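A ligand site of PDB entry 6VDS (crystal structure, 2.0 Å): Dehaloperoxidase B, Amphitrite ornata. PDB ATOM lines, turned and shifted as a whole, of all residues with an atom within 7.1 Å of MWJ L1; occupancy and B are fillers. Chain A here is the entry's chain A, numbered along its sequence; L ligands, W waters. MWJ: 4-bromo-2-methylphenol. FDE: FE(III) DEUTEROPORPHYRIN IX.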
ATOM      1  N   PHE A  21     -27.079 -22.521  30.861  1.00  0.00           N
ATOM      2  CA  PHE A  21     -25.744 -23.146  30.777  1.00  0.00           C
ATOM      3  C   PHE A  21     -25.831 -24.497  31.453  1.00  0.00           C
ATOM      4  O   PHE A  21     -25.231 -25.428  30.897  1.00  0.00           O
ATOM      5  CB  PHE A  21     -24.681 -22.231  31.364  1.00  0.00           C
ATOM      6  CG  PHE A  21     -23.315 -22.559  30.821  1.00  0.00           C
ATOM      7  CD1 PHE A  21     -23.094 -22.509  29.461  1.00  0.00           C
ATOM      8  CD2 PHE A  21     -22.286 -22.960  31.658  1.00  0.00           C
ATOM      9  CE1 PHE A  21     -21.844 -22.801  28.938  1.00  0.00           C
ATOM     10  CE2 PHE A  21     -21.028 -23.225  31.131  1.00  0.00           C
ATOM     11  CZ  PHE A  21     -20.823 -23.169  29.778  1.00  0.00           C
ATOM     12  N   PHE A  24     -27.465 -26.813  29.227  1.00  0.00           N
ATOM     13  CA  PHE A  24     -26.439 -27.233  28.223  1.00  0.00           C
ATOM     14  C   PHE A  24     -25.590 -28.355  28.804  1.00  0.00           C
ATOM     15  O   PHE A  24     -25.469 -29.421  28.136  1.00  0.00           O
ATOM     16  CB  PHE A  24     -25.645 -26.036  27.710  1.00  0.00           C
ATOM     17  CG  PHE A  24     -24.306 -26.366  27.082  1.00  0.00           C
ATOM     18  CD1 PHE A  24     -24.209 -27.075  25.893  1.00  0.00           C
ATOM     19  CD2 PHE A  24     -23.137 -25.918  27.679  1.00  0.00           C
ATOM     20  CE1 PHE A  24     -22.970 -27.283  25.303  1.00  0.00           C
ATOM     21  CE2 PHE A  24     -21.887 -26.163  27.116  1.00  0.00           C
ATOM     22  CZ  PHE A  24     -21.813 -26.836  25.918  1.00  0.00           C
ATOM     23  N   GLU A  31     -19.529 -32.101  27.930  1.00  0.00           N
ATOM     24  CA  GLU A  31     -19.029 -30.698  27.851  1.00  0.00           C
ATOM     25  C   GLU A  31     -18.315 -30.263  29.141  1.00  0.00           C
ATOM     26  O   GLU A  31     -17.423 -29.367  29.057  1.00  0.00           O
ATOM     27  CB  GLU A  31     -20.176 -29.738  27.546  1.00  0.00           C
ATOM     28  CG  GLU A  31     -20.891 -30.075  26.269  1.00  0.00           C
ATOM     29  CD  GLU A  31     -20.149 -29.744  24.987  1.00  0.00           C
ATOM     30  OE1 GLU A  31     -20.529 -30.322  23.975  1.00  0.00           O
ATOM     31  OE2 GLU A  31     -19.185 -28.930  25.007  1.00  0.00           O
ATOM     32  N   ARG A  33     -16.029 -31.475  30.790  1.00  0.00           N
ATOM     33  CA  ARG A  33     -14.574 -31.794  30.765  1.00  0.00           C
ATOM     34  C   ARG A  33     -13.787 -30.618  30.185  1.00  0.00           C
ATOM     35  O   ARG A  33     -12.564 -30.575  30.388  1.00  0.00           O
ATOM     36  CB  ARG A  33     -14.352 -33.077  29.959  1.00  0.00           C
ATOM     37  CG  ARG A  33     -15.129 -34.287  30.461  1.00  0.00           C
ATOM     38  CD  ARG A  33     -15.748 -35.046  29.294  1.00  0.00           C
ATOM     39  NE  ARG A  33     -15.787 -36.491  29.443  1.00  0.00           N
ATOM     40  CZ  ARG A  33     -16.077 -37.343  28.469  1.00  0.00           C
ATOM     41  NH1 ARG A  33     -16.381 -36.886  27.259  1.00  0.00           N
ATOM     42  NH2 ARG A  33     -16.063 -38.654  28.687  1.00  0.00           N
ATOM     43  N   ASN A  34     -14.440 -29.677  29.498  1.00  0.00           N
ATOM     44  CA  ASN A  34     -13.792 -28.444  28.994  1.00  0.00           C
ATOM     45  C   ASN A  34     -13.599 -27.466  30.162  1.00  0.00           C
ATOM     46  O   ASN A  34     -12.768 -26.543  30.033  1.00  0.00           O
ATOM     47  CB  ASN A  34     -14.588 -27.878  27.814  1.00  0.00           C
ATOM     48  CG  ASN A  34     -14.584 -28.852  26.664  1.00  0.00           C
ATOM     49  OD1 ASN A  34     -13.521 -29.354  26.278  1.00  0.00           O
ATOM     50  ND2 ASN A  34     -15.761 -29.184  26.147  1.00  0.00           N
ATOM     51  N   PHE A  35     -14.324 -27.713  31.266  1.00  0.00           N
ATOM     52  CA  PHE A  35     -14.309 -26.979  32.569  1.00  0.00           C
ATOM     53  C   PHE A  35     -14.100 -27.994  33.716  1.00  0.00           C
ATOM     54  O   PHE A  35     -14.882 -27.991  34.673  1.00  0.00           O
ATOM     55  CB  PHE A  35     -15.639 -26.207  32.706  1.00  0.00           C
ATOM     56  CG  PHE A  35     -16.248 -25.625  31.439  1.00  0.00           C
ATOM     57  CD1 PHE A  35     -17.106 -26.365  30.644  1.00  0.00           C
ATOM     58  CD2 PHE A  35     -16.025 -24.309  31.093  1.00  0.00           C
ATOM     59  CE1 PHE A  35     -17.691 -25.810  29.512  1.00  0.00           C
ATOM     60  CE2 PHE A  35     -16.608 -23.732  29.965  1.00  0.00           C
ATOM     61  CZ  PHE A  35     -17.453 -24.489  29.182  1.00  0.00           C
ATOM     62  N   HIS A  55     -17.910 -16.707  35.138  1.00  0.00           N
ATOM     63  CA  HIS A  55     -17.610 -17.114  33.743  1.00  0.00           C
ATOM     64  C   HIS A  55     -18.895 -17.235  32.947  1.00  0.00           C
ATOM     65  O   HIS A  55     -18.894 -16.752  31.819  1.00  0.00           O
ATOM     66  CB  HIS A  55     -16.784 -18.391  33.616  1.00  0.00           C
ATOM     67  CG  HIS A  55     -16.310 -18.611  32.221  1.00  0.00           C
ATOM     68  ND1 HIS A  55     -16.981 -19.450  31.358  1.00  0.00           N
ATOM     69  CD2 HIS A  55     -15.253 -18.125  31.547  1.00  0.00           C
ATOM     70  CE1 HIS A  55     -16.358 -19.491  30.209  1.00  0.00           C
ATOM     71  NE2 HIS A  55     -15.289 -18.671  30.277  1.00  0.00           N
ATOM     72  N   VAL A  59     -19.794 -15.125  29.568  1.00  0.00           N
ATOM     73  CA  VAL A  59     -20.200 -15.803  28.295  1.00  0.00           C
ATOM     74  C   VAL A  59     -21.417 -15.085  27.718  1.00  0.00           C
ATOM     75  O   VAL A  59     -21.431 -14.782  26.488  1.00  0.00           O
ATOM     76  CB  VAL A  59     -20.508 -17.299  28.480  1.00  0.00           C
ATOM     77  CG1 VAL A  59     -21.079 -17.871  27.192  1.00  0.00           C
ATOM     78  CG2 VAL A  59     -19.262 -18.085  28.924  1.00  0.00           C
ATOM     79  N   HIS A  89      -8.718 -18.659  24.483  1.00  0.00           N
ATOM     80  CA  HIS A  89      -9.907 -19.370  23.927  1.00  0.00           C
ATOM     81  C   HIS A  89      -9.587 -20.002  22.561  1.00  0.00           C
ATOM     82  O   HIS A  89     -10.542 -20.396  21.884  1.00  0.00           O
ATOM     83  CB  HIS A  89     -11.112 -18.421  23.882  1.00  0.00           C
ATOM     84  CG  HIS A  89     -11.598 -18.068  25.245  1.00  0.00           C
ATOM     85  ND1 HIS A  89     -10.959 -17.126  26.023  1.00  0.00           N
ATOM     86  CD2 HIS A  89     -12.645 -18.521  25.968  1.00  0.00           C
ATOM     87  CE1 HIS A  89     -11.596 -17.001  27.163  1.00  0.00           C
ATOM     88  NE2 HIS A  89     -12.620 -17.862  27.162  1.00  0.00           N
ATOM     89  N   GLY A  91      -8.979 -22.886  21.812  1.00  0.00           N
ATOM     90  CA  GLY A  91      -9.574 -24.242  21.740  1.00  0.00           C
ATOM     91  C   GLY A  91     -11.104 -24.294  21.710  1.00  0.00           C
ATOM     92  O   GLY A  91     -11.640 -25.391  21.897  1.00  0.00           O
ATOM     93  N   LEU A  92     -11.808 -23.179  21.471  1.00  0.00           N
ATOM     94  CA  LEU A  92     -13.296 -23.211  21.280  1.00  0.00           C
ATOM     95  C   LEU A  92     -13.634 -23.915  19.954  1.00  0.00           C
ATOM     96  O   LEU A  92     -12.810 -23.836  19.033  1.00  0.00           O
ATOM     97  CB  LEU A  92     -13.841 -21.779  21.277  1.00  0.00           C
ATOM     98  CG  LEU A  92     -13.674 -20.986  22.572  1.00  0.00           C
ATOM     99  CD1 LEU A  92     -14.313 -19.606  22.406  1.00  0.00           C
ATOM    100  CD2 LEU A  92     -14.283 -21.716  23.758  1.00  0.00           C
ATOM    101  N   THR A  93     -14.794 -24.578  19.851  1.00  0.00           N
ATOM    102  CA  THR A  93     -15.250 -25.225  18.589  1.00  0.00           C
ATOM    103  C   THR A  93     -16.725 -24.915  18.319  1.00  0.00           C
ATOM    104  O   THR A  93     -17.475 -24.714  19.270  1.00  0.00           O
ATOM    105  CB  THR A  93     -15.076 -26.745  18.514  1.00  0.00           C
ATOM    106  OG1 THR A  93     -16.089 -27.379  19.296  1.00  0.00           O
ATOM    107  CG2 THR A  93     -13.705 -27.234  18.955  1.00  0.00           C
ATOM    108  N   THR A  94     -17.097 -24.921  17.035  1.00  0.00           N
ATOM    109  CA  THR A  94     -18.406 -24.465  16.532  1.00  0.00           C
ATOM    110  C   THR A  94     -19.458 -25.506  16.930  1.00  0.00           C
ATOM    111  O   THR A  94     -20.529 -25.087  17.338  1.00  0.00           O
ATOM    112  CB  THR A  94     -18.334 -24.144  15.040  1.00  0.00           C
ATOM    113  OG1 THR A  94     -18.022 -25.343  14.341  1.00  0.00           O
ATOM    114  CG2 THR A  94     -17.314 -23.060  14.737  1.00  0.00           C
ATOM    115  N   GLY A  95     -19.100 -26.804  16.921  1.00  0.00           N
ATOM    116  CA  GLY A  95     -19.979 -27.910  17.370  1.00  0.00           C
ATOM    117  C   GLY A  95     -20.431 -27.735  18.809  1.00  0.00           C
ATOM    118  O   GLY A  95     -21.602 -28.080  19.101  1.00  0.00           O
ATOM    119  N   ASN A  96     -19.557 -27.221  19.675  1.00  0.00           N
ATOM    120  CA  ASN A  96     -19.858 -26.891  21.102  1.00  0.00           C
ATOM    121  C   ASN A  96     -20.834 -25.704  21.170  1.00  0.00           C
ATOM    122  O   ASN A  96     -21.724 -25.761  22.052  1.00  0.00           O
ATOM    123  CB  ASN A  96     -18.596 -26.635  21.919  1.00  0.00           C
ATOM    124  CG  ASN A  96     -17.645 -27.823  21.904  1.00  0.00           C
ATOM    125  OD1 ASN A  96     -16.433 -27.650  21.698  1.00  0.00           O
ATOM    126  ND2 ASN A  96     -18.182 -29.022  22.044  1.00  0.00           N
ATOM    127  N   PHE A  97     -20.708 -24.692  20.303  1.00  0.00           N
ATOM    128  CA  PHE A  97     -21.674 -23.564  20.216  1.00  0.00           C
ATOM    129  C   PHE A  97     -23.054 -24.087  19.776  1.00  0.00           C
ATOM    130  O   PHE A  97     -24.039 -23.709  20.422  1.00  0.00           O
ATOM    131  CB  PHE A  97     -21.142 -22.426  19.332  1.00  0.00           C
ATOM    132  CG  PHE A  97     -20.212 -21.464  20.054  1.00  0.00           C
ATOM    133  CD1 PHE A  97     -20.720 -20.494  20.897  1.00  0.00           C
ATOM    134  CD2 PHE A  97     -18.841 -21.547  19.880  1.00  0.00           C
ATOM    135  CE1 PHE A  97     -19.877 -19.592  21.530  1.00  0.00           C
ATOM    136  CE2 PHE A  97     -17.998 -20.645  20.513  1.00  0.00           C
ATOM    137  CZ  PHE A  97     -18.514 -19.676  21.334  1.00  0.00           C
ATOM    138  N   GLU A  98     -23.132 -24.954  18.758  1.00  0.00           N
ATOM    139  CA  GLU A  98     -24.425 -25.497  18.241  1.00  0.00           C
ATOM    140  C   GLU A  98     -25.140 -26.224  19.385  1.00  0.00           C
ATOM    141  O   GLU A  98     -26.343 -25.999  19.536  1.00  0.00           O
ATOM    142  CB  GLU A  98     -24.259 -26.434  17.045  1.00  0.00           C
ATOM    143  CG  GLU A  98     -25.498 -26.505  16.159  1.00  0.00           C
ATOM    144  N   LEU A 100     -24.649 -25.487  22.659  1.00  0.00           N
ATOM    145  CA  LEU A 100     -25.138 -24.428  23.555  1.00  0.00           C
ATOM    146  C   LEU A 100     -26.489 -23.955  23.029  1.00  0.00           C
ATOM    147  O   LEU A 100     -27.436 -23.865  23.821  1.00  0.00           O
ATOM    148  CB  LEU A 100     -24.135 -23.264  23.675  1.00  0.00           C
ATOM    149  CG  LEU A 100     -24.574 -22.107  24.582  1.00  0.00           C
ATOM    150  CD1 LEU A 100     -24.821 -22.531  26.030  1.00  0.00           C
ATOM    151  CD2 LEU A 100     -23.527 -20.989  24.554  1.00  0.00           C
ATOM    152  N   MET A 136     -12.845 -20.755  13.115  1.00  0.00           N
ATOM    153  CA  MET A 136     -13.056 -21.693  14.269  1.00  0.00           C
ATOM    154  C   MET A 136     -13.343 -23.088  13.703  1.00  0.00           C
ATOM    155  O   MET A 136     -14.182 -23.157  12.810  1.00  0.00           O
ATOM    156  CB  MET A 136     -14.219 -21.274  15.187  1.00  0.00           C
ATOM    157  CG  MET A 136     -14.223 -22.011  16.530  1.00  0.00           C
ATOM    158  SD  MET A 136     -15.563 -21.539  17.701  1.00  0.00           S
ATOM    159  CE  MET A 136     -14.849 -20.092  18.485  1.00  0.00           C
HETATM  160  C4  MWJ L   1     -17.361 -23.631  22.728  1.00  0.00           C
HETATM  161  C1  MWJ L   1     -16.039 -25.986  25.404  1.00  0.00           C
HETATM  162  C7  MWJ L   1     -17.982 -24.384  25.318  1.00  0.00           C
HETATM  163  C2  MWJ L   1     -16.876 -24.959  24.687  1.00  0.00           C
HETATM  164  C6  MWJ L   1     -18.756 -23.451  24.643  1.00  0.00           C
HETATM  165  C3  MWJ L   1     -16.572 -24.571  23.379  1.00  0.00           C
HETATM  166  C5  MWJ L   1     -18.456 -23.075  23.354  1.00  0.00           C
HETATM  167 BR1  MWJ L   1     -20.251 -22.666  25.525  1.00  0.00          BR
HETATM  168  O1  MWJ L   1     -15.502 -25.122  22.736  1.00  0.00           O
HETATM  169  CHA FDE L   2     -11.644 -20.123  29.920  1.00  0.00           C
HETATM  170  C1A FDE L   2     -11.725 -18.728  30.341  1.00  0.00           C
HETATM  171  C2A FDE L   2     -10.823 -18.127  31.371  1.00  0.00           C
HETATM  172  CAA FDE L   2      -9.760 -18.821  32.198  1.00  0.00           C
HETATM  173  CBA FDE L   2     -10.415 -19.870  33.089  1.00  0.00           C
HETATM  174  CGA FDE L   2     -10.498 -19.495  34.552  1.00  0.00           C
HETATM  175  O1A FDE L   2     -10.890 -18.348  34.888  1.00  0.00           O
HETATM  176  O2A FDE L   2     -10.156 -20.373  35.387  1.00  0.00           O
HETATM  177  C3A FDE L   2     -11.226 -16.700  31.485  1.00  0.00           C
HETATM  178  CMA FDE L   2     -10.633 -15.693  32.439  1.00  0.00           C
HETATM  179  C4A FDE L   2     -12.365 -16.522  30.509  1.00  0.00           C
HETATM  180  NA  FDE L   2     -12.548 -17.734  29.686  1.00  0.00           N
HETATM  181  CHB FDE L   2     -13.039 -15.241  30.239  1.00  0.00           C
HETATM  182  C1B FDE L   2     -14.098 -15.078  29.215  1.00  0.00           C
HETATM  183  C2B FDE L   2     -14.573 -13.801  28.959  1.00  0.00           C
HETATM  184  C3B FDE L   2     -15.495 -14.006  27.968  1.00  0.00           C
HETATM  185  CME FDE L   2     -16.236 -12.806  27.431  1.00  0.00           C
HETATM  186  C4B FDE L   2     -15.479 -15.454  27.678  1.00  0.00           C
HETATM  187  NB  FDE L   2     -14.608 -16.089  28.478  1.00  0.00           N
HETATM  188  CHC FDE L   2     -16.324 -16.126  26.688  1.00  0.00           C
HETATM  189  C1C FDE L   2     -16.401 -17.578  26.513  1.00  0.00           C
HETATM  190  C2C FDE L   2     -17.352 -18.050  25.629  1.00  0.00           C
HETATM  191  C3C FDE L   2     -17.184 -19.407  25.717  1.00  0.00           C
HETATM  192  CMF FDE L   2     -18.082 -20.239  24.863  1.00  0.00           C
HETATM  193  C4C FDE L   2     -16.110 -19.648  26.696  1.00  0.00           C
HETATM  194  NC  FDE L   2     -15.657 -18.482  27.169  1.00  0.00           N
HETATM  195  CHD FDE L   2     -15.577 -20.968  27.088  1.00  0.00           C
HETATM  196  C1D FDE L   2     -14.376 -21.184  27.908  1.00  0.00           C
HETATM  197  C2D FDE L   2     -13.777 -22.543  28.086  1.00  0.00           C
HETATM  198  CMD FDE L   2     -14.247 -23.866  27.556  1.00  0.00           C
HETATM  199  C3D FDE L   2     -12.603 -22.281  28.924  1.00  0.00           C
HETATM  200  CAD FDE L   2     -11.581 -23.259  29.458  1.00  0.00           C
HETATM  201  CBD FDE L   2     -11.633 -23.382  30.980  1.00  0.00           C
HETATM  202  CGD FDE L   2     -10.350 -23.988  31.530  1.00  0.00           C
HETATM  203  O1D FDE L   2     -10.442 -24.744  32.513  1.00  0.00           O
HETATM  204  O2D FDE L   2      -9.250 -23.726  30.994  1.00  0.00           O
HETATM  205  C4D FDE L   2     -12.653 -20.813  29.109  1.00  0.00           C
HETATM  206  ND  FDE L   2     -13.697 -20.185  28.521  1.00  0.00           N
HETATM  207 FE   FDE L   2     -14.144 -18.126  28.545  1.00  0.00          FE
HETATM  208  O   HOH W   1     -14.005 -27.084  22.523  1.00  0.00           O
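The side-chain amide oxygen (OD1) of Asn 96 sits at hydrogen-bond distance from an oxygen (O1) of MWJ L1, 2.9 Å away.
N of Thr 93 lies within hydrogen-bond range of O1 of MWJ L1, 3.0 Å away.
NE2 of His 55 binds FE of FDE L2 (2.1 Å).
An iron atom (FE) of FDE L2 is bound by a ring nitrogen (NE2) of His 89.
The side-chain hydroxyl (OG1) of Thr 93 lies within hydrogen-bond range of the side-chain amide oxygen (OD1) of Asn 96 (2.4 Å).
The side-chain amide nitrogen of Asn 96 lies within hydrogen-bond range of the side-chain carboxylate of Glu 31, 3.1 Å away.
The side-chain amide nitrogen of Asn 34 is in hydrogen-bond range of the backbone carbonyl oxygen of Glu 31 (3.4 Å).
Phe 21 touches MWJ L1.
Asn 34 touches MWJ L1.
CZ of Phe 35 touches C7 of MWJ L1 (3.9 Å).
Gly 91 touches MWJ L1 (O to O1, 3.96 Å).
Leu 92 touches MWJ L1.
Phe 97 touches MWJ L1.
CD2 of Leu 100 touches BR1 of MWJ L1, 3.8 Å away.
Hydrophobic or aromatic side chains within 4 Å of MWJ L1: Phe 21, Phe 35, Leu 92, Phe 97 and Leu 100.
Nine residues have an atom within 4 Å of MWJ L1: Phe 21, Asn 34, Phe 35, Gly 91, Leu 92, Thr 93, Asn 96, Phe 97 and Leu 100.
The nearest printed residue that does not touch MWJ L1 is Phe 24 (4.2 Å).
Water W1 lies within hydrogen-bond range of an oxygen (O1) of MWJ L1 (2.5 Å), the side-chain amide oxygen (OD1) of Asn 96 (2.6 Å) and the backbone carbonyl oxygen (O) of Gly 91 (3.0 Å).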
